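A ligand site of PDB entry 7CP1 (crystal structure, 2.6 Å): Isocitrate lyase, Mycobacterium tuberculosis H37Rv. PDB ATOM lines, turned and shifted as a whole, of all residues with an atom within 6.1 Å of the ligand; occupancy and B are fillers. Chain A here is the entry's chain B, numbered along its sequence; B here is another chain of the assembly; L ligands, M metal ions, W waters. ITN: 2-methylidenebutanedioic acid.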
ATOM      1  N   TYR A  89     -32.274 -24.600  -5.052  1.00  0.00           N
ATOM      2  CA  TYR A  89     -30.858 -24.877  -4.792  1.00  0.00           C
ATOM      3  C   TYR A  89     -30.715 -26.286  -4.245  1.00  0.00           C
ATOM      4  O   TYR A  89     -31.434 -26.693  -3.324  1.00  0.00           O
ATOM      5  CB  TYR A  89     -30.225 -23.871  -3.828  1.00  0.00           C
ATOM      6  CG  TYR A  89     -28.786 -24.229  -3.553  1.00  0.00           C
ATOM      7  CD1 TYR A  89     -27.822 -24.076  -4.531  1.00  0.00           C
ATOM      8  CD2 TYR A  89     -28.400 -24.789  -2.325  1.00  0.00           C
ATOM      9  CE1 TYR A  89     -26.506 -24.458  -4.314  1.00  0.00           C
ATOM     10  CE2 TYR A  89     -27.084 -25.159  -2.101  1.00  0.00           C
ATOM     11  CZ  TYR A  89     -26.126 -24.989  -3.095  1.00  0.00           C
ATOM     12  OH  TYR A  89     -24.798 -25.351  -2.881  1.00  0.00           O
ATOM     13  N   SER A  91     -28.159 -28.474  -2.450  1.00  0.00           N
ATOM     14  CA  SER A  91     -26.956 -28.551  -1.631  1.00  0.00           C
ATOM     15  C   SER A  91     -26.326 -29.950  -1.691  1.00  0.00           C
ATOM     16  O   SER A  91     -26.984 -30.948  -1.379  1.00  0.00           O
ATOM     17  CB  SER A  91     -27.316 -28.209  -0.180  1.00  0.00           C
ATOM     18  OG  SER A  91     -26.169 -28.189   0.635  1.00  0.00           O
ATOM     19  N   GLY A  92     -25.043 -30.018  -2.057  1.00  0.00           N
ATOM     20  CA  GLY A  92     -24.329 -31.274  -1.887  1.00  0.00           C
ATOM     21  C   GLY A  92     -24.101 -31.606  -0.423  1.00  0.00           C
ATOM     22  O   GLY A  92     -24.067 -32.787  -0.041  1.00  0.00           O
ATOM     23  N   TRP A  93     -23.954 -30.582   0.425  1.00  0.00           N
ATOM     24  CA  TRP A  93     -23.880 -30.790   1.870  1.00  0.00           C
ATOM     25  C   TRP A  93     -25.105 -31.531   2.378  1.00  0.00           C
ATOM     26  O   TRP A  93     -24.992 -32.514   3.132  1.00  0.00           O
ATOM     27  CB  TRP A  93     -23.732 -29.439   2.580  1.00  0.00           C
ATOM     28  CG  TRP A  93     -23.371 -29.478   4.064  1.00  0.00           C
ATOM     29  CD1 TRP A  93     -22.208 -29.056   4.628  1.00  0.00           C
ATOM     30  CD2 TRP A  93     -24.200 -29.933   5.167  1.00  0.00           C
ATOM     31  NE1 TRP A  93     -22.237 -29.223   5.991  1.00  0.00           N
ATOM     32  CE2 TRP A  93     -23.445 -29.763   6.353  1.00  0.00           C
ATOM     33  CE3 TRP A  93     -25.498 -30.448   5.265  1.00  0.00           C
ATOM     34  CZ2 TRP A  93     -23.933 -30.108   7.616  1.00  0.00           C
ATOM     35  CZ3 TRP A  93     -25.988 -30.800   6.540  1.00  0.00           C
ATOM     36  CH2 TRP A  93     -25.204 -30.612   7.684  1.00  0.00           C
ATOM     37  N   ASP A 108     -19.322 -33.039   4.942  1.00  0.00           N
ATOM     38  CA  ASP A 108     -19.229 -32.389   3.631  1.00  0.00           C
ATOM     39  C   ASP A 108     -17.793 -32.481   3.100  1.00  0.00           C
ATOM     40  O   ASP A 108     -17.041 -31.502   3.083  1.00  0.00           O
ATOM     41  CB  ASP A 108     -19.735 -30.960   3.737  1.00  0.00           C
ATOM     42  CG  ASP A 108     -19.754 -30.213   2.401  1.00  0.00           C
ATOM     43  OD1 ASP A 108     -19.840 -30.863   1.329  1.00  0.00           O
ATOM     44  OD2 ASP A 108     -19.652 -28.962   2.435  1.00  0.00           O
ATOM     45  N   ASP A 153     -25.156 -28.452  -6.685  1.00  0.00           N
ATOM     46  CA  ASP A 153     -23.799 -28.474  -6.167  1.00  0.00           C
ATOM     47  C   ASP A 153     -23.005 -29.566  -6.888  1.00  0.00           C
ATOM     48  O   ASP A 153     -23.324 -30.752  -6.790  1.00  0.00           O
ATOM     49  CB  ASP A 153     -23.882 -28.701  -4.652  1.00  0.00           C
ATOM     50  CG  ASP A 153     -22.543 -28.649  -3.926  1.00  0.00           C
ATOM     51  OD1 ASP A 153     -21.468 -28.685  -4.580  1.00  0.00           O
ATOM     52  OD2 ASP A 153     -22.593 -28.591  -2.668  1.00  0.00           O
ATOM     53  N   GLU A 155     -19.628 -29.861  -6.284  1.00  0.00           N
ATOM     54  CA  GLU A 155     -18.438 -30.095  -5.437  1.00  0.00           C
ATOM     55  C   GLU A 155     -17.225 -29.704  -6.274  1.00  0.00           C
ATOM     56  O   GLU A 155     -17.259 -28.656  -6.946  1.00  0.00           O
ATOM     57  CB  GLU A 155     -18.408 -31.536  -4.892  1.00  0.00           C
ATOM     58  CG  GLU A 155     -19.724 -32.068  -4.288  1.00  0.00           C
ATOM     59  CD  GLU A 155     -19.928 -31.659  -2.837  1.00  0.00           C
ATOM     60  OE1 GLU A 155     -19.178 -30.780  -2.344  1.00  0.00           O
ATOM     61  OE2 GLU A 155     -20.846 -32.217  -2.185  1.00  0.00           O
ATOM     62  N   HIS A 180     -22.557 -25.594  -9.897  1.00  0.00           N
ATOM     63  CA  HIS A 180     -21.404 -24.848  -9.410  1.00  0.00           C
ATOM     64  C   HIS A 180     -20.238 -25.777  -9.076  1.00  0.00           C
ATOM     65  O   HIS A 180     -20.423 -26.957  -8.776  1.00  0.00           O
ATOM     66  CB  HIS A 180     -21.780 -23.948  -8.215  1.00  0.00           C
ATOM     67  CG  HIS A 180     -22.231 -24.651  -6.966  1.00  0.00           C
ATOM     68  ND1 HIS A 180     -21.364 -25.324  -6.135  1.00  0.00           N
ATOM     69  CD2 HIS A 180     -23.444 -24.696  -6.357  1.00  0.00           C
ATOM     70  CE1 HIS A 180     -22.018 -25.780  -5.094  1.00  0.00           C
ATOM     71  NE2 HIS A 180     -23.286 -25.406  -5.195  1.00  0.00           N
ATOM     72  N   GLU A 182     -16.102 -25.880  -7.406  1.00  0.00           N
ATOM     73  CA  GLU A 182     -15.184 -25.198  -6.515  1.00  0.00           C
ATOM     74  C   GLU A 182     -13.754 -25.688  -6.690  1.00  0.00           C
ATOM     75  O   GLU A 182     -13.506 -26.795  -7.181  1.00  0.00           O
ATOM     76  CB  GLU A 182     -15.621 -25.363  -5.049  1.00  0.00           C
ATOM     77  CG  GLU A 182     -15.719 -26.800  -4.581  1.00  0.00           C
ATOM     78  CD  GLU A 182     -16.686 -26.950  -3.427  1.00  0.00           C
ATOM     79  OE1 GLU A 182     -17.855 -26.519  -3.556  1.00  0.00           O
ATOM     80  OE2 GLU A 182     -16.275 -27.495  -2.377  1.00  0.00           O
ATOM     81  N   ARG A 228     -16.792 -21.362  -8.016  1.00  0.00           N
ATOM     82  CA  ARG A 228     -16.645 -21.027  -6.607  1.00  0.00           C
ATOM     83  C   ARG A 228     -15.170 -21.086  -6.236  1.00  0.00           C
ATOM     84  O   ARG A 228     -14.441 -21.989  -6.683  1.00  0.00           O
ATOM     85  CB  ARG A 228     -17.442 -21.986  -5.732  1.00  0.00           C
ATOM     86  CG  ARG A 228     -17.014 -21.997  -4.274  1.00  0.00           C
ATOM     87  CD  ARG A 228     -17.866 -22.949  -3.432  1.00  0.00           C
ATOM     88  NE  ARG A 228     -17.166 -23.354  -2.209  1.00  0.00           N
ATOM     89  CZ  ARG A 228     -17.750 -24.013  -1.206  1.00  0.00           C
ATOM     90  NH1 ARG A 228     -19.040 -24.327  -1.255  1.00  0.00           N
ATOM     91  NH2 ARG A 228     -17.035 -24.334  -0.139  1.00  0.00           N
ATOM     92  N   TRP A 283     -18.541 -16.991  -7.373  1.00  0.00           N
ATOM     93  CA  TRP A 283     -18.973 -17.134  -5.985  1.00  0.00           C
ATOM     94  C   TRP A 283     -17.745 -17.259  -5.097  1.00  0.00           C
ATOM     95  O   TRP A 283     -16.979 -18.222  -5.226  1.00  0.00           O
ATOM     96  CB  TRP A 283     -19.892 -18.349  -5.853  1.00  0.00           C
ATOM     97  CG  TRP A 283     -20.208 -18.842  -4.457  1.00  0.00           C
ATOM     98  CD1 TRP A 283     -20.121 -18.146  -3.280  1.00  0.00           C
ATOM     99  CD2 TRP A 283     -20.694 -20.159  -4.113  1.00  0.00           C
ATOM    100  NE1 TRP A 283     -20.517 -18.944  -2.228  1.00  0.00           N
ATOM    101  CE2 TRP A 283     -20.868 -20.179  -2.711  1.00  0.00           C
ATOM    102  CE3 TRP A 283     -20.989 -21.310  -4.860  1.00  0.00           C
ATOM    103  CZ2 TRP A 283     -21.329 -21.322  -2.030  1.00  0.00           C
ATOM    104  CZ3 TRP A 283     -21.459 -22.442  -4.184  1.00  0.00           C
ATOM    105  CH2 TRP A 283     -21.620 -22.433  -2.787  1.00  0.00           C
ATOM    106  N   GLU A 285     -16.792 -18.199  -1.594  1.00  0.00           N
ATOM    107  CA  GLU A 285     -17.284 -18.779  -0.364  1.00  0.00           C
ATOM    108  C   GLU A 285     -16.776 -17.973   0.829  1.00  0.00           C
ATOM    109  O   GLU A 285     -15.582 -17.696   0.943  1.00  0.00           O
ATOM    110  CB  GLU A 285     -16.843 -20.242  -0.253  1.00  0.00           C
ATOM    111  CG  GLU A 285     -16.765 -20.758   1.201  1.00  0.00           C
ATOM    112  CD  GLU A 285     -18.107 -21.285   1.735  1.00  0.00           C
ATOM    113  OE1 GLU A 285     -19.129 -21.163   1.042  1.00  0.00           O
ATOM    114  OE2 GLU A 285     -18.127 -21.824   2.852  1.00  0.00           O
ATOM    115  N   THR A 286     -17.687 -17.585   1.714  1.00  0.00           N
ATOM    116  CA  THR A 286     -17.296 -16.745   2.835  1.00  0.00           C
ATOM    117  C   THR A 286     -17.937 -17.235   4.118  1.00  0.00           C
ATOM    118  O   THR A 286     -19.074 -17.714   4.131  1.00  0.00           O
ATOM    119  CB  THR A 286     -17.680 -15.268   2.594  1.00  0.00           C
ATOM    120  OG1 THR A 286     -17.145 -14.468   3.646  1.00  0.00           O
ATOM    121  CG2 THR A 286     -19.178 -15.067   2.581  1.00  0.00           C
ATOM    122  N   ASN A 313     -23.726 -17.239  -1.167  1.00  0.00           N
ATOM    123  CA  ASN A 313     -24.360 -18.089  -0.165  1.00  0.00           C
ATOM    124  C   ASN A 313     -24.485 -17.302   1.127  1.00  0.00           C
ATOM    125  O   ASN A 313     -23.493 -16.738   1.611  1.00  0.00           O
ATOM    126  CB  ASN A 313     -23.569 -19.388   0.072  1.00  0.00           C
ATOM    127  CG  ASN A 313     -24.142 -20.258   1.227  1.00  0.00           C
ATOM    128  OD1 ASN A 313     -25.371 -20.359   1.438  1.00  0.00           O
ATOM    129  ND2 ASN A 313     -23.249 -20.889   1.989  1.00  0.00           N
ATOM    130  N   CYS A 314     -25.686 -17.265   1.695  1.00  0.00           N
ATOM    131  CA  CYS A 314     -25.870 -16.626   2.994  1.00  0.00           C
ATOM    132  C   CYS A 314     -25.720 -17.690   4.060  1.00  0.00           C
ATOM    133  O   CYS A 314     -26.519 -18.636   4.112  1.00  0.00           O
ATOM    134  CB  CYS A 314     -27.217 -15.934   3.058  1.00  0.00           C
ATOM    135  SG  CYS A 314     -27.501 -14.796   1.653  1.00  0.00           S
ATOM    136  N   SER A 315     -24.727 -17.531   4.915  1.00  0.00           N
ATOM    137  CA  SER A 315     -24.246 -18.589   5.799  1.00  0.00           C
ATOM    138  C   SER A 315     -25.347 -19.073   6.723  1.00  0.00           C
ATOM    139  O   SER A 315     -25.906 -18.264   7.478  1.00  0.00           O
ATOM    140  CB  SER A 315     -23.060 -18.092   6.631  1.00  0.00           C
ATOM    141  OG  SER A 315     -22.725 -18.993   7.677  1.00  0.00           O
ATOM    142  N   PRO A 316     -25.680 -20.369   6.711  1.00  0.00           N
ATOM    143  CA  PRO A 316     -26.686 -20.864   7.666  1.00  0.00           C
ATOM    144  C   PRO A 316     -26.144 -21.065   9.069  1.00  0.00           C
ATOM    145  O   PRO A 316     -26.952 -21.140  10.002  1.00  0.00           O
ATOM    146  CB  PRO A 316     -27.098 -22.208   7.054  1.00  0.00           C
ATOM    147  CG  PRO A 316     -25.871 -22.665   6.307  1.00  0.00           C
ATOM    148  CD  PRO A 316     -25.202 -21.407   5.792  1.00  0.00           C
ATOM    149  N   PHE A 345     -28.541 -17.673  -2.052  1.00  0.00           N
ATOM    150  CA  PHE A 345     -29.160 -18.894  -1.579  1.00  0.00           C
ATOM    151  C   PHE A 345     -28.707 -19.185  -0.158  1.00  0.00           C
ATOM    152  O   PHE A 345     -27.652 -18.729   0.293  1.00  0.00           O
ATOM    153  CB  PHE A 345     -28.837 -20.078  -2.519  1.00  0.00           C
ATOM    154  CG  PHE A 345     -27.351 -20.247  -2.801  1.00  0.00           C
ATOM    155  CD1 PHE A 345     -26.697 -19.427  -3.707  1.00  0.00           C
ATOM    156  CD2 PHE A 345     -26.623 -21.247  -2.171  1.00  0.00           C
ATOM    157  CE1 PHE A 345     -25.337 -19.590  -3.971  1.00  0.00           C
ATOM    158  CE2 PHE A 345     -25.264 -21.420  -2.432  1.00  0.00           C
ATOM    159  CZ  PHE A 345     -24.612 -20.585  -3.322  1.00  0.00           C
ATOM    160  N   THR A 347     -27.633 -22.486   1.755  1.00  0.00           N
ATOM    161  CA  THR A 347     -27.299 -23.869   1.436  1.00  0.00           C
ATOM    162  C   THR A 347     -28.111 -24.879   2.270  1.00  0.00           C
ATOM    163  O   THR A 347     -28.592 -25.877   1.731  1.00  0.00           O
ATOM    164  CB  THR A 347     -25.795 -24.112   1.619  1.00  0.00           C
ATOM    165  OG1 THR A 347     -25.306 -23.417   2.775  1.00  0.00           O
ATOM    166  CG2 THR A 347     -25.033 -23.651   0.387  1.00  0.00           C
ATOM    167  N   LEU A 348     -28.254 -24.645   3.578  1.00  0.00           N
ATOM    168  CA  LEU A 348     -28.751 -25.694   4.459  1.00  0.00           C
ATOM    169  C   LEU A 348     -30.181 -25.459   4.943  1.00  0.00           C
ATOM    170  O   LEU A 348     -30.585 -25.965   6.001  1.00  0.00           O
ATOM    171  CB  LEU A 348     -27.797 -25.863   5.645  1.00  0.00           C
ATOM    172  CG  LEU A 348     -26.383 -26.269   5.256  1.00  0.00           C
ATOM    173  CD1 LEU A 348     -25.637 -26.871   6.456  1.00  0.00           C
ATOM    174  CD2 LEU A 348     -26.378 -27.259   4.059  1.00  0.00           C
ATOM    175  N   HIS B 393     -24.256 -28.238  13.040  1.00  0.00           N
ATOM    176  CA  HIS B 393     -24.600 -29.027  11.851  1.00  0.00           C
ATOM    177  C   HIS B 393     -23.479 -29.964  11.423  1.00  0.00           C
ATOM    178  O   HIS B 393     -23.746 -31.127  11.052  1.00  0.00           O
ATOM    179  CB  HIS B 393     -24.976 -28.083  10.713  1.00  0.00           C
ATOM    180  CG  HIS B 393     -23.844 -27.222  10.240  1.00  0.00           C
ATOM    181  ND1 HIS B 393     -23.166 -26.371  11.095  1.00  0.00           N
ATOM    182  CD2 HIS B 393     -23.264 -27.090   9.030  1.00  0.00           C
ATOM    183  CE1 HIS B 393     -22.218 -25.751  10.412  1.00  0.00           C
ATOM    184  NE2 HIS B 393     -22.258 -26.171   9.160  1.00  0.00           N
ATOM    185  N   GLN B 394     -22.232 -29.483  11.419  1.00  0.00           N
ATOM    186  CA  GLN B 394     -21.134 -30.358  11.023  1.00  0.00           C
ATOM    187  C   GLN B 394     -21.062 -31.567  11.934  1.00  0.00           C
ATOM    188  O   GLN B 394     -21.024 -32.710  11.466  1.00  0.00           O
ATOM    189  CB  GLN B 394     -19.808 -29.587  11.051  1.00  0.00           C
ATOM    190  CG  GLN B 394     -19.850 -28.251  10.332  1.00  0.00           C
ATOM    191  CD  GLN B 394     -19.944 -28.394   8.798  1.00  0.00           C
ATOM    192  OE1 GLN B 394     -20.666 -29.252   8.273  1.00  0.00           O
ATOM    193  NE2 GLN B 394     -19.244 -27.529   8.088  1.00  0.00           N
HETATM  194  C1  ITN L   1     -21.368 -26.031   0.955  1.00  0.00           C
HETATM  195  C2  ITN L   1     -22.402 -25.952   2.089  1.00  0.00           C
HETATM  196  C3  ITN L   1     -22.323 -24.787   3.108  1.00  0.00           C
HETATM  197  C5  ITN L   1     -21.846 -23.350   2.783  1.00  0.00           C
HETATM  198  O3  ITN L   1     -22.009 -22.453   3.671  1.00  0.00           O
HETATM  199  O4  ITN L   1     -21.307 -23.025   1.672  1.00  0.00           O
HETATM  200  C4  ITN L   1     -22.716 -25.005   4.333  1.00  0.00           C
HETATM  201  O1  ITN L   1     -21.735 -26.057  -0.251  1.00  0.00           O
HETATM  202  O2  ITN L   1     -20.138 -26.105   1.169  1.00  0.00           O
HETATM  203 MG    MG M   1     -20.898 -29.399  -0.683  1.00  0.00          MG
HETATM  204  O   HOH W   1     -23.996 -27.138  -0.264  1.00  0.00           O
HETATM  205  O   HOH W   2     -17.819 -27.558   0.078  1.00  0.00           O
HETATM  206  O   HOH W   3     -20.212 -27.138  -2.448  1.00  0.00           O
HETATM  207  O   HOH W   4     -20.957 -25.103   6.574  1.00  0.00           O
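The side-chain amide nitrogen (ND2) of Asn 313 is in hydrogen-bond range of an oxygen (O3) of the ligand (2.6 Å). O4 of the ligand sits close to OE1 of Glu 285 (2.9 Å). An oxygen (O2) of the ligand lies within salt-bridge range of the guanidinium group of Arg 228, at 3.2 Å.
The side-chain amide oxygen (OD1) of Asn 313 is in hydrogen-bond range of the backbone NH (N) of Thr 347, 3.1 Å away. The side-chain amide oxygen of Asn 313 lies close to the backbone carbonyl oxygen of Phe 345, 3.0 Å away. The guanidinium group (NH1) of Arg 228 lies within salt-bridge range of the side-chain carboxylate (OE1) of Glu 285 (3.9 Å). The guanidinium group (NH1) of Arg 228 is in salt-bridge range of the side-chain carboxylate (OE1) of Glu 182 (3.4 Å). OD2 of Asp 153 lies within hydrogen-bond range of N of Gly 92 (2.9 Å). The backbone NH (N) of Glu 155 sits at hydrogen-bond distance from the side-chain carboxylate (OD1) of Asp 153 (2.8 Å). The backbone NH (N) of Trp 93 sits close to the side-chain hydroxyl (OG) of Ser 91. The side-chain amide oxygen (OE1) of Gln 394 of chain B sits at hydrogen-bond distance from the indole nitrogen (NE1) of Trp 93, 2.8 Å away.
An oxygen (O2) of the ligand sits close to the side-chain carboxylate (OD2) of Asp 108. CB of Trp 93 touches C2 of the ligand (3.8 Å). Asp 153 touches the ligand (OD2 to O1, 3.6 Å). Pro 316 touches the ligand. Thr 347 touches the ligand (OG1 to C3, 3.3 Å). CG of Leu 348 touches C4 of the ligand, 3.99 Å away. Hydrophobic or aromatic side chains within 4 Å of the ligand: Trp 93, Pro 316 and Leu 348. Of the 22 residues printed, 9 come within 4 Å of the ligand.
Water W1 lies within hydrogen-bond range of O1 of the ligand (2.5 Å), OG of Ser 91 (2.6 Å), OD2 of Asp 153 (3.1 Å) and OH of Tyr 89 (3.3 Å). Water W4 lies within hydrogen-bond range of a ring nitrogen (NE2) of His 393 of chain B (3.1 Å) and the side-chain amide nitrogen of Gln 394 of chain B (3.3 Å). Water W3 lies within hydrogen-bond range of OE1 of Glu 182 (2.7 Å), OD2 of Asp 153 (2.8 Å), O1 of the ligand (2.9 Å) and NH1 of Arg 228 (3.3 Å). Water W2 lies within hydrogen-bond range of OE2 of Glu 182 (2.9 Å), O2 of the ligand (2.9 Å), OD2 of Asp 108 (3.3 Å) and NH2 of Arg 228 (3.3 Å).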
